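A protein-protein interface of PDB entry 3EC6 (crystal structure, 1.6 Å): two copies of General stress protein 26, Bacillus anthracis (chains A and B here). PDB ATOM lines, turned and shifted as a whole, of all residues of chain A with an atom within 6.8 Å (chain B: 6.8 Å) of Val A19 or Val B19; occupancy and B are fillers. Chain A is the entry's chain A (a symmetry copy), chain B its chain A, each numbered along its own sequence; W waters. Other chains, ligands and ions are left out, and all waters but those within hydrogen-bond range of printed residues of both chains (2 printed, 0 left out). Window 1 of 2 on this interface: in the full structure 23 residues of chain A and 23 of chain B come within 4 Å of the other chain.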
ATOM      1  N   ARG A  16      30.330  16.855 -10.558  1.00  0.00           N
ATOM      2  CA  ARG A  16      30.070  17.708 -11.698  1.00  0.00           C
ATOM      3  C   ARG A  16      29.389  19.056 -11.362  1.00  0.00           C
ATOM      4  O   ARG A  16      29.469  19.970 -12.154  1.00  0.00           O
ATOM      5  CB  ARG A  16      29.228  16.933 -12.734  1.00  0.00           C
ATOM      6  CG  ARG A  16      30.063  16.189 -13.791  1.00  0.00           C
ATOM      7  CD  ARG A  16      29.198  15.542 -14.852  1.00  0.00           C
ATOM      8  NE  ARG A  16      29.976  14.483 -15.484  1.00  0.00           N
ATOM      9  CZ  ARG A  16      29.811  13.187 -15.221  1.00  0.00           C
ATOM     10  NH1 ARG A  16      28.829  12.796 -14.399  1.00  0.00           N
ATOM     11  NH2 ARG A  16      30.594  12.265 -15.820  1.00  0.00           N
ATOM     12  N   THR A  17      28.701  19.180 -10.228  1.00  0.00           N
ATOM     13  CA  THR A  17      27.887  20.401  -9.978  1.00  0.00           C
ATOM     14  C   THR A  17      28.739  21.531  -9.445  1.00  0.00           C
ATOM     15  O   THR A  17      29.440  21.355  -8.464  1.00  0.00           O
ATOM     16  CB  THR A  17      26.656  20.193  -9.047  1.00  0.00           C
ATOM     17  OG1 THR A  17      25.823  19.148  -9.588  1.00  0.00           O
ATOM     18  CG2 THR A  17      25.877  21.485  -8.952  1.00  0.00           C
ATOM     19  N   GLY A  18      28.690  22.675 -10.112  1.00  0.00           N
ATOM     20  CA  GLY A  18      29.408  23.868  -9.691  1.00  0.00           C
ATOM     21  C   GLY A  18      28.501  25.074  -9.840  1.00  0.00           C
ATOM     22  O   GLY A  18      27.280  24.934 -10.062  1.00  0.00           O
ATOM     23  N   VAL A  19      29.100  26.264  -9.807  1.00  0.00           N
ATOM     24  CA  VAL A  19      28.353  27.510  -9.956  1.00  0.00           C
ATOM     25  C   VAL A  19      28.899  28.271 -11.143  1.00  0.00           C
ATOM     26  O   VAL A  19      30.114  28.465 -11.214  1.00  0.00           O
ATOM     27  CB  VAL A  19      28.528  28.389  -8.709  1.00  0.00           C
ATOM     28  CG1 VAL A  19      27.768  29.667  -8.871  1.00  0.00           C
ATOM     29  CG2 VAL A  19      28.023  27.601  -7.432  1.00  0.00           C
ATOM     30  N   LEU A  20      28.021  28.667 -12.068  1.00  0.00           N
ATOM     31  CA  LEU A  20      28.417  29.509 -13.199  1.00  0.00           C
ATOM     32  C   LEU A  20      27.889  30.907 -12.946  1.00  0.00           C
ATOM     33  O   LEU A  20      26.654  31.093 -12.824  1.00  0.00           O
ATOM     34  CB  LEU A  20      27.754  28.950 -14.471  1.00  0.00           C
ATOM     35  CG  LEU A  20      27.958  29.779 -15.757  1.00  0.00           C
ATOM     36  CD1 LEU A  20      29.465  29.915 -16.121  1.00  0.00           C
ATOM     37  CD2 LEU A  20      27.193  29.160 -16.972  1.00  0.00           C
ATOM     38  N   SER A  21      28.795  31.874 -12.873  1.00  0.00           N
ATOM     39  CA  SER A  21      28.359  33.275 -12.658  1.00  0.00           C
ATOM     40  C   SER A  21      28.622  34.085 -13.925  1.00  0.00           C
ATOM     41  O   SER A  21      29.627  33.925 -14.623  1.00  0.00           O
ATOM     42  CB  SER A  21      29.191  33.872 -11.533  1.00  0.00           C
ATOM     43  OG  SER A  21      29.021  33.042 -10.375  1.00  0.00           O
ATOM     44  N   HIS A  29      24.930  37.400 -11.611  1.00  0.00           N
ATOM     45  CA  HIS A  29      23.958  36.306 -11.541  1.00  0.00           C
ATOM     46  C   HIS A  29      24.713  35.006 -11.469  1.00  0.00           C
ATOM     47  O   HIS A  29      25.647  34.782 -12.249  1.00  0.00           O
ATOM     48  CB  HIS A  29      23.082  36.269 -12.772  1.00  0.00           C
ATOM     49  CG  HIS A  29      22.087  35.153 -12.724  1.00  0.00           C
ATOM     50  ND1 HIS A  29      22.355  33.882 -13.205  1.00  0.00           N
ATOM     51  CD2 HIS A  29      20.830  35.109 -12.209  1.00  0.00           C
ATOM     52  CE1 HIS A  29      21.289  33.117 -13.019  1.00  0.00           C
ATOM     53  NE2 HIS A  29      20.349  33.844 -12.420  1.00  0.00           N
ATOM     54  N   SER A  30      24.251  34.102 -10.624  1.00  0.00           N
ATOM     55  CA  SER A  30      24.907  32.810 -10.470  1.00  0.00           C
ATOM     56  C   SER A  30      23.871  31.702 -10.528  1.00  0.00           C
ATOM     57  O   SER A  30      22.785  31.843 -10.012  1.00  0.00           O
ATOM     58  CB  SER A  30      25.622  32.718  -9.134  1.00  0.00           C
ATOM     59  OG  SER A  30      26.738  33.583  -9.114  1.00  0.00           O
ATOM     60  N   ALA A  31      24.258  30.569 -11.096  1.00  0.00           N
ATOM     61  CA  ALA A  31      23.353  29.420 -11.198  1.00  0.00           C
ATOM     62  C   ALA A  31      24.168  28.155 -10.958  1.00  0.00           C
ATOM     63  O   ALA A  31      25.335  28.056 -11.375  1.00  0.00           O
ATOM     64  CB  ALA A  31      22.701  29.368 -12.588  1.00  0.00           C
ATOM     65  N   PHE A  32      23.559  27.181 -10.302  1.00  0.00           N
ATOM     66  CA  PHE A  32      24.140  25.831 -10.264  1.00  0.00           C
ATOM     67  C   PHE A  32      24.056  25.230 -11.660  1.00  0.00           C
ATOM     68  O   PHE A  32      23.027  25.331 -12.329  1.00  0.00           O
ATOM     69  CB  PHE A  32      23.399  24.938  -9.231  1.00  0.00           C
ATOM     70  CG  PHE A  32      23.499  25.468  -7.827  1.00  0.00           C
ATOM     71  CD1 PHE A  32      24.714  25.415  -7.162  1.00  0.00           C
ATOM     72  CD2 PHE A  32      22.384  26.053  -7.191  1.00  0.00           C
ATOM     73  CE1 PHE A  32      24.841  25.927  -5.876  1.00  0.00           C
ATOM     74  CE2 PHE A  32      22.504  26.550  -5.881  1.00  0.00           C
ATOM     75  CZ  PHE A  32      23.724  26.469  -5.239  1.00  0.00           C
ATOM     76  N   MET A  33      25.118  24.551 -12.074  1.00  0.00           N
ATOM     77  CA  MET A  33      25.194  23.918 -13.407  1.00  0.00           C
ATOM     78  C   MET A  33      26.097  22.677 -13.272  1.00  0.00           C
ATOM     79  O   MET A  33      27.028  22.657 -12.423  1.00  0.00           O
ATOM     80  CB  MET A  33      25.757  24.843 -14.516  1.00  0.00           C
ATOM     81  CG  MET A  33      25.034  26.184 -14.599  1.00  0.00           C
ATOM     82  SD  MET A  33      23.261  26.028 -15.302  1.00  0.00           S
ATOM     83  CE  MET A  33      23.538  26.562 -17.103  1.00  0.00           C
ATOM     84  N   PHE A  35      29.070  20.529 -14.800  1.00  0.00           N
ATOM     85  CA  PHE A  35      30.203  20.851 -15.665  1.00  0.00           C
ATOM     86  C   PHE A  35      30.859  19.639 -16.286  1.00  0.00           C
ATOM     87  O   PHE A  35      31.242  18.686 -15.564  1.00  0.00           O
ATOM     88  CB  PHE A  35      31.276  21.654 -14.865  1.00  0.00           C
ATOM     89  CG  PHE A  35      30.875  23.057 -14.586  1.00  0.00           C
ATOM     90  CD1 PHE A  35      31.285  24.095 -15.423  1.00  0.00           C
ATOM     91  CD2 PHE A  35      30.024  23.334 -13.483  1.00  0.00           C
ATOM     92  CE1 PHE A  35      30.867  25.447 -15.152  1.00  0.00           C
ATOM     93  CE2 PHE A  35      29.595  24.677 -13.258  1.00  0.00           C
ATOM     94  CZ  PHE A  35      30.018  25.714 -14.072  1.00  0.00           C
ATOM     95  N   HIS A  63      32.632  33.341 -14.501  1.00  0.00           N
ATOM     96  CA  HIS A  63      33.403  32.880 -13.346  1.00  0.00           C
ATOM     97  C   HIS A  63      32.783  31.544 -12.934  1.00  0.00           C
ATOM     98  O   HIS A  63      31.560  31.385 -12.967  1.00  0.00           O
ATOM     99  CB  HIS A  63      33.271  33.917 -12.237  1.00  0.00           C
ATOM    100  CG  HIS A  63      34.060  33.598 -11.014  1.00  0.00           C
ATOM    101  ND1 HIS A  63      33.561  32.764 -10.026  1.00  0.00           N
ATOM    102  CD2 HIS A  63      35.321  33.915 -10.653  1.00  0.00           C
ATOM    103  CE1 HIS A  63      34.469  32.638  -9.074  1.00  0.00           C
ATOM    104  NE2 HIS A  63      35.551  33.326  -9.423  1.00  0.00           N
ATOM    105  N   VAL A  64      33.612  30.569 -12.595  1.00  0.00           N
ATOM    106  CA  VAL A  64      33.164  29.229 -12.162  1.00  0.00           C
ATOM    107  C   VAL A  64      33.759  28.902 -10.809  1.00  0.00           C
ATOM    108  O   VAL A  64      34.923  29.109 -10.600  1.00  0.00           O
ATOM    109  CB  VAL A  64      33.593  28.163 -13.199  1.00  0.00           C
ATOM    110  CG1 VAL A  64      33.278  26.753 -12.696  1.00  0.00           C
ATOM    111  CG2 VAL A  64      32.915  28.407 -14.533  1.00  0.00           C
ATOM    112  N   LEU A  65      32.917  28.377  -9.914  1.00  0.00           N
ATOM    113  CA  LEU A  65      33.338  27.735  -8.663  1.00  0.00           C
ATOM    114  C   LEU A  65      33.004  26.270  -8.820  1.00  0.00           C
ATOM    115  O   LEU A  65      31.871  25.909  -9.167  1.00  0.00           O
ATOM    116  CB  LEU A  65      32.609  28.278  -7.413  1.00  0.00           C
ATOM    117  CG  LEU A  65      32.828  29.735  -7.136  1.00  0.00           C
ATOM    118  CD1 LEU A  65      31.906  30.125  -5.989  1.00  0.00           C
ATOM    119  CD2 LEU A  65      34.283  29.883  -6.643  1.00  0.00           C
ATOM    120  N   LEU A  66      33.994  25.396  -8.608  1.00  0.00           N
ATOM    121  CA  LEU A  66      33.751  23.942  -8.840  1.00  0.00           C
ATOM    122  C   LEU A  66      34.591  23.091  -7.904  1.00  0.00           C
ATOM    123  O   LEU A  66      35.761  23.364  -7.695  1.00  0.00           O
ATOM    124  CB  LEU A  66      34.099  23.573 -10.300  1.00  0.00           C
ATOM    125  CG  LEU A  66      33.910  22.126 -10.765  1.00  0.00           C
ATOM    126  CD1 LEU A  66      32.416  21.795 -10.822  1.00  0.00           C
ATOM    127  CD2 LEU A  66      34.510  21.981 -12.158  1.00  0.00           C
ATOM    128  N   ARG B  16      24.317  27.140   6.625  1.00  0.00           N
ATOM    129  CA  ARG B  16      24.755  28.514   6.495  1.00  0.00           C
ATOM    130  C   ARG B  16      25.568  28.820   5.214  1.00  0.00           C
ATOM    131  O   ARG B  16      25.653  29.967   4.830  1.00  0.00           O
ATOM    132  CB  ARG B  16      25.566  28.911   7.746  1.00  0.00           C
ATOM    133  CG  ARG B  16      24.722  29.544   8.866  1.00  0.00           C
ATOM    134  CD  ARG B  16      25.574  30.025  10.022  1.00  0.00           C
ATOM    135  NE  ARG B  16      24.720  30.129  11.199  1.00  0.00           N
ATOM    136  CZ  ARG B  16      24.710  29.233  12.187  1.00  0.00           C
ATOM    137  NH1 ARG B  16      25.580  28.216  12.168  1.00  0.00           N
ATOM    138  NH2 ARG B  16      23.865  29.378  13.229  1.00  0.00           N
ATOM    139  N   THR B  17      26.187  27.828   4.576  1.00  0.00           N
ATOM    140  CA  THR B  17      27.122  28.129   3.457  1.00  0.00           C
ATOM    141  C   THR B  17      26.377  28.341   2.158  1.00  0.00           C
ATOM    142  O   THR B  17      25.595  27.496   1.760  1.00  0.00           O
ATOM    143  CB  THR B  17      28.253  27.079   3.244  1.00  0.00           C
ATOM    144  OG1 THR B  17      28.989  26.919   4.472  1.00  0.00           O
ATOM    145  CG2 THR B  17      29.173  27.552   2.141  1.00  0.00           C
ATOM    146  N   GLY B  18      26.609  29.480   1.523  1.00  0.00           N
ATOM    147  CA  GLY B  18      26.012  29.804   0.236  1.00  0.00           C
ATOM    148  C   GLY B  18      27.065  30.428  -0.659  1.00  0.00           C
ATOM    149  O   GLY B  18      28.272  30.401  -0.342  1.00  0.00           O
ATOM    150  N   VAL B  19      26.611  31.068  -1.737  1.00  0.00           N
ATOM    151  CA  VAL B  19      27.512  31.731  -2.677  1.00  0.00           C
ATOM    152  C   VAL B  19      27.143  33.195  -2.759  1.00  0.00           C
ATOM    153  O   VAL B  19      25.967  33.499  -2.973  1.00  0.00           O
ATOM    154  CB  VAL B  19      27.357  31.124  -4.079  1.00  0.00           C
ATOM    155  CG1 VAL B  19      28.275  31.813  -5.039  1.00  0.00           C
ATOM    156  CG2 VAL B  19      27.677  29.575  -4.022  1.00  0.00           C
ATOM    157  N   LEU B  20      28.123  34.081  -2.566  1.00  0.00           N
ATOM    158  CA  LEU B  20      27.909  35.520  -2.737  1.00  0.00           C
ATOM    159  C   LEU B  20      28.583  35.941  -4.028  1.00  0.00           C
ATOM    160  O   LEU B  20      29.819  35.782  -4.165  1.00  0.00           O
ATOM    161  CB  LEU B  20      28.586  36.250  -1.562  1.00  0.00           C
ATOM    162  CG  LEU B  20      28.571  37.792  -1.629  1.00  0.00           C
ATOM    163  CD1 LEU B  20      27.119  38.353  -1.663  1.00  0.00           C
ATOM    164  CD2 LEU B  20      29.337  38.430  -0.426  1.00  0.00           C
ATOM    165  N   SER B  21      27.796  36.472  -4.955  1.00  0.00           N
ATOM    166  CA  SER B  21      28.381  36.938  -6.236  1.00  0.00           C
ATOM    167  C   SER B  21      28.304  38.461  -6.300  1.00  0.00           C
ATOM    168  O   SER B  21      27.337  39.100  -5.875  1.00  0.00           O
ATOM    169  CB  SER B  21      27.551  36.373  -7.379  1.00  0.00           C
ATOM    170  OG  SER B  21      27.541  34.945  -7.248  1.00  0.00           O
ATOM    171  N   HIS B  29      32.200  37.699 -10.070  1.00  0.00           N
ATOM    172  CA  HIS B  29      33.027  36.973  -9.103  1.00  0.00           C
ATOM    173  C   HIS B  29      32.119  36.350  -8.077  1.00  0.00           C
ATOM    174  O   HIS B  29      31.220  37.019  -7.551  1.00  0.00           O
ATOM    175  CB  HIS B  29      33.974  37.905  -8.381  1.00  0.00           C
ATOM    176  CG  HIS B  29      34.823  37.184  -7.382  1.00  0.00           C
ATOM    177  ND1 HIS B  29      34.438  36.991  -6.065  1.00  0.00           N
ATOM    178  CD2 HIS B  29      36.027  36.571  -7.522  1.00  0.00           C
ATOM    179  CE1 HIS B  29      35.389  36.320  -5.432  1.00  0.00           C
ATOM    180  NE2 HIS B  29      36.366  36.059  -6.297  1.00  0.00           N
ATOM    181  N   SER B  30      32.409  35.118  -7.702  1.00  0.00           N
ATOM    182  CA  SER B  30      31.595  34.416  -6.720  1.00  0.00           C
ATOM    183  C   SER B  30      32.492  33.786  -5.670  1.00  0.00           C
ATOM    184  O   SER B  30      33.549  33.284  -5.980  1.00  0.00           O
ATOM    185  CB  SER B  30      30.784  33.311  -7.372  1.00  0.00           C
ATOM    186  OG  SER B  30      29.781  33.862  -8.200  1.00  0.00           O
ATOM    187  N   ALA B  31      32.012  33.751  -4.435  1.00  0.00           N
ATOM    188  CA  ALA B  31      32.778  33.154  -3.336  1.00  0.00           C
ATOM    189  C   ALA B  31      31.802  32.411  -2.431  1.00  0.00           C
ATOM    190  O   ALA B  31      30.663  32.859  -2.213  1.00  0.00           O
ATOM    191  CB  ALA B  31      33.512  34.240  -2.537  1.00  0.00           C
ATOM    192  N   PHE B  32      32.243  31.288  -1.890  1.00  0.00           N
ATOM    193  CA  PHE B  32      31.504  30.648  -0.793  1.00  0.00           C
ATOM    194  C   PHE B  32      31.610  31.533   0.441  1.00  0.00           C
ATOM    195  O   PHE B  32      32.687  32.033   0.767  1.00  0.00           O
ATOM    196  CB  PHE B  32      32.060  29.226  -0.505  1.00  0.00           C
ATOM    197  CG  PHE B  32      31.929  28.301  -1.683  1.00  0.00           C
ATOM    198  CD1 PHE B  32      30.674  27.851  -2.061  1.00  0.00           C
ATOM    199  CD2 PHE B  32      33.059  27.916  -2.433  1.00  0.00           C
ATOM    200  CE1 PHE B  32      30.521  27.020  -3.165  1.00  0.00           C
ATOM    201  CE2 PHE B  32      32.910  27.057  -3.537  1.00  0.00           C
ATOM    202  CZ  PHE B  32      31.648  26.613  -3.879  1.00  0.00           C
ATOM    203  N   MET B  33      30.506  31.673   1.162  1.00  0.00           N
ATOM    204  CA  MET B  33      30.445  32.507   2.381  1.00  0.00           C
ATOM    205  C   MET B  33      29.393  31.878   3.313  1.00  0.00           C
ATOM    206  O   MET B  33      28.411  31.252   2.833  1.00  0.00           O
ATOM    207  CB  MET B  33      30.074  33.989   2.117  1.00  0.00           C
ATOM    208  CG  MET B  33      30.957  34.646   1.060  1.00  0.00           C
ATOM    209  SD  MET B  33      32.742  34.958   1.673  1.00  0.00           S
ATOM    210  CE  MET B  33      32.656  36.802   2.118  1.00  0.00           C
ATOM    211  N   PHE B  35      26.296  32.466   5.731  1.00  0.00           N
ATOM    212  CA  PHE B  35      25.271  33.505   5.820  1.00  0.00           C
ATOM    213  C   PHE B  35      24.519  33.507   7.131  1.00  0.00           C
ATOM    214  O   PHE B  35      23.975  32.457   7.552  1.00  0.00           O
ATOM    215  CB  PHE B  35      24.250  33.350   4.650  1.00  0.00           C
ATOM    216  CG  PHE B  35      24.796  33.767   3.333  1.00  0.00           C
ATOM    217  CD1 PHE B  35      24.572  35.054   2.843  1.00  0.00           C
ATOM    218  CD2 PHE B  35      25.597  32.859   2.589  1.00  0.00           C
ATOM    219  CE1 PHE B  35      25.130  35.449   1.575  1.00  0.00           C
ATOM    220  CE2 PHE B  35      26.168  33.288   1.353  1.00  0.00           C
ATOM    221  CZ  PHE B  35      25.928  34.557   0.852  1.00  0.00           C
ATOM    222  N   HIS B  63      24.283  39.062  -5.642  1.00  0.00           N
ATOM    223  CA  HIS B  63      23.385  37.934  -5.891  1.00  0.00           C
ATOM    224  C   HIS B  63      23.810  36.837  -4.914  1.00  0.00           C
ATOM    225  O   HIS B  63      25.006  36.638  -4.678  1.00  0.00           O
ATOM    226  CB  HIS B  63      23.564  37.488  -7.337  1.00  0.00           C
ATOM    227  CG  HIS B  63      22.661  36.375  -7.743  1.00  0.00           C
ATOM    228  ND1 HIS B  63      22.988  35.050  -7.499  1.00  0.00           N
ATOM    229  CD2 HIS B  63      21.425  36.375  -8.285  1.00  0.00           C
ATOM    230  CE1 HIS B  63      22.008  34.280  -7.940  1.00  0.00           C
ATOM    231  NE2 HIS B  63      21.043  35.053  -8.425  1.00  0.00           N
ATOM    232  N   VAL B  64      22.850  36.157  -4.309  1.00  0.00           N
ATOM    233  CA  VAL B  64      23.103  35.060  -3.351  1.00  0.00           C
ATOM    234  C   VAL B  64      22.382  33.808  -3.803  1.00  0.00           C
ATOM    235  O   VAL B  64      21.240  33.872  -4.167  1.00  0.00           O
ATOM    236  CB  VAL B  64      22.621  35.466  -1.937  1.00  0.00           C
ATOM    237  CG1 VAL B  64      22.730  34.290  -0.965  1.00  0.00           C
ATOM    238  CG2 VAL B  64      23.413  36.650  -1.418  1.00  0.00           C
ATOM    239  N   LEU B  65      23.092  32.677  -3.753  1.00  0.00           N
ATOM    240  CA  LEU B  65      22.512  31.334  -3.871  1.00  0.00           C
ATOM    241  C   LEU B  65      22.678  30.694  -2.513  1.00  0.00           C
ATOM    242  O   LEU B  65      23.781  30.674  -1.949  1.00  0.00           O
ATOM    243  CB  LEU B  65      23.214  30.448  -4.926  1.00  0.00           C
ATOM    244  CG  LEU B  65      23.153  30.967  -6.330  1.00  0.00           C
ATOM    245  CD1 LEU B  65      24.034  30.069  -7.188  1.00  0.00           C
ATOM    246  CD2 LEU B  65      21.696  30.793  -6.808  1.00  0.00           C
ATOM    247  N   LEU B  66      21.579  30.192  -1.940  1.00  0.00           N
ATOM    248  CA  LEU B  66      21.660  29.633  -0.559  1.00  0.00           C
ATOM    249  C   LEU B  66      20.663  28.504  -0.366  1.00  0.00           C
ATOM    250  O   LEU B  66      19.523  28.602  -0.786  1.00  0.00           O
ATOM    251  CB  LEU B  66      21.372  30.740   0.479  1.00  0.00           C
ATOM    252  CG  LEU B  66      21.417  30.390   1.970  1.00  0.00           C
ATOM    253  CD1 LEU B  66      22.861  30.094   2.385  1.00  0.00           C
ATOM    254  CD2 LEU B  66      20.901  31.583   2.765  1.00  0.00           C
HETATM  255  O   HOH W   1      25.433  33.933  -6.010  1.00  0.00           O
HETATM  256  O   HOH W   2      30.903  31.221  -9.997  1.00  0.00           O
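OG of Ser B21 sits at hydrogen-bond distance from OG of Ser A30, 2.4 Å away.
The side-chain hydroxyl (OG) of Ser A21 lies within hydrogen-bond range of the side-chain hydroxyl (OG) of Ser B30 (2.4 Å).
The side-chain hydroxyl (OG) of Ser A30 is in hydrogen-bond range of the side-chain hydroxyl (OG) of Ser B30, at 3.2 Å.
N of Val B19 is in hydrogen-bond range of O of Leu B65 (2.9 Å).
N of Ser B21 lies within hydrogen-bond range of O of His B63 (2.8 Å).
The backbone NH of Val A19 is in hydrogen-bond range of the backbone carbonyl oxygen of Leu A65 (2.9 Å).
The backbone carbonyl oxygen (O) of Ala A31 lies within hydrogen-bond range of the backbone NH (N) of Leu A20 (2.8 Å).
OG of Ser A21 lies within hydrogen-bond range of OG of Ser A30.
The backbone carbonyl oxygen (O) of His A63 is in hydrogen-bond range of the backbone NH (N) of Ser A21.
Among the printed residues, merely in contact across the chains: Val A19 with Val B19 (3.96 Å), Ser A21 with Ser B21 (3.9 Å), His A29 with His B63 (3.8 Å), Ser A30 with His B63 (3.3 Å), Ser A30 with Leu B65 (3.5 Å), Ala A31 with Leu B65 (3.9 Å), His A63 with His B29 (3.8 Å), His A63 with Ser B30 (3.3 Å), Leu A65 with Ser B30 (3.5 Å) and Leu A65 with Ala B31 (3.9 Å).
Printed residues of chain B within 4 Å of Ser A30: Ser B21, Ser B30, His B63 and Leu B65.
Of the printed residues of chain B, Leu A65 touches Ser B30 (3.5 Å) and Ala B31 (3.9 Å).
The nearest residue of chain B that does not touch Val A19 is Leu B65 (4.1 Å).
The nearest residue of chain A that does not touch Val B19 is Leu A65 (4.1 Å).
Hydrophobic or aromatic side chains of chain A within 4 Å of the printed part of chain B: Val A19, His A29, His A63 and Leu A65.
Of the 16 printed residues of chain B, 7 touch a printed residue of chain A.
Among the printed residues, 13 pairs touch across the chains.
Among the printed residues, no Asp or Glu carboxylate lies within 4 Å of a Lys or Arg side-chain nitrogen of the other chain.
Ser A21 touches its own counterpart, Ser B21.
His A29 touches His B63, and with the chains exchanged His A63 touches His B29.
Ser B30 touches its own counterpart, Ser A30.
Ala A31 touches Leu B65, and with the chains exchanged Leu A65 touches Ala B31.
Positions printed for both chains: 16, 17, 18, 19, 20, 21, 29, 30, 31, 32, 33, 35, 63, 64, 65 and 66.
Water W1 lies within hydrogen-bond range of the side-chain hydroxyl (OG) of Ser B21 (2.6 Å), the backbone carbonyl oxygen (O) of His B63 (3.0 Å), the backbone carbonyl oxygen (O) of Val B19 (3.1 Å), the side-chain hydroxyl (OG) of Ser A30 (3.4 Å) and the backbone NH (N) of Leu B65 (3.5 Å).
Water W2 lies within hydrogen-bond range of the side-chain hydroxyl (OG) of Ser A21, the backbone carbonyl oxygen (O) of His A63, the backbone carbonyl oxygen (O) of Val A19, the side-chain hydroxyl (OG) of Ser B30 and the backbone NH (N) of Leu A65.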
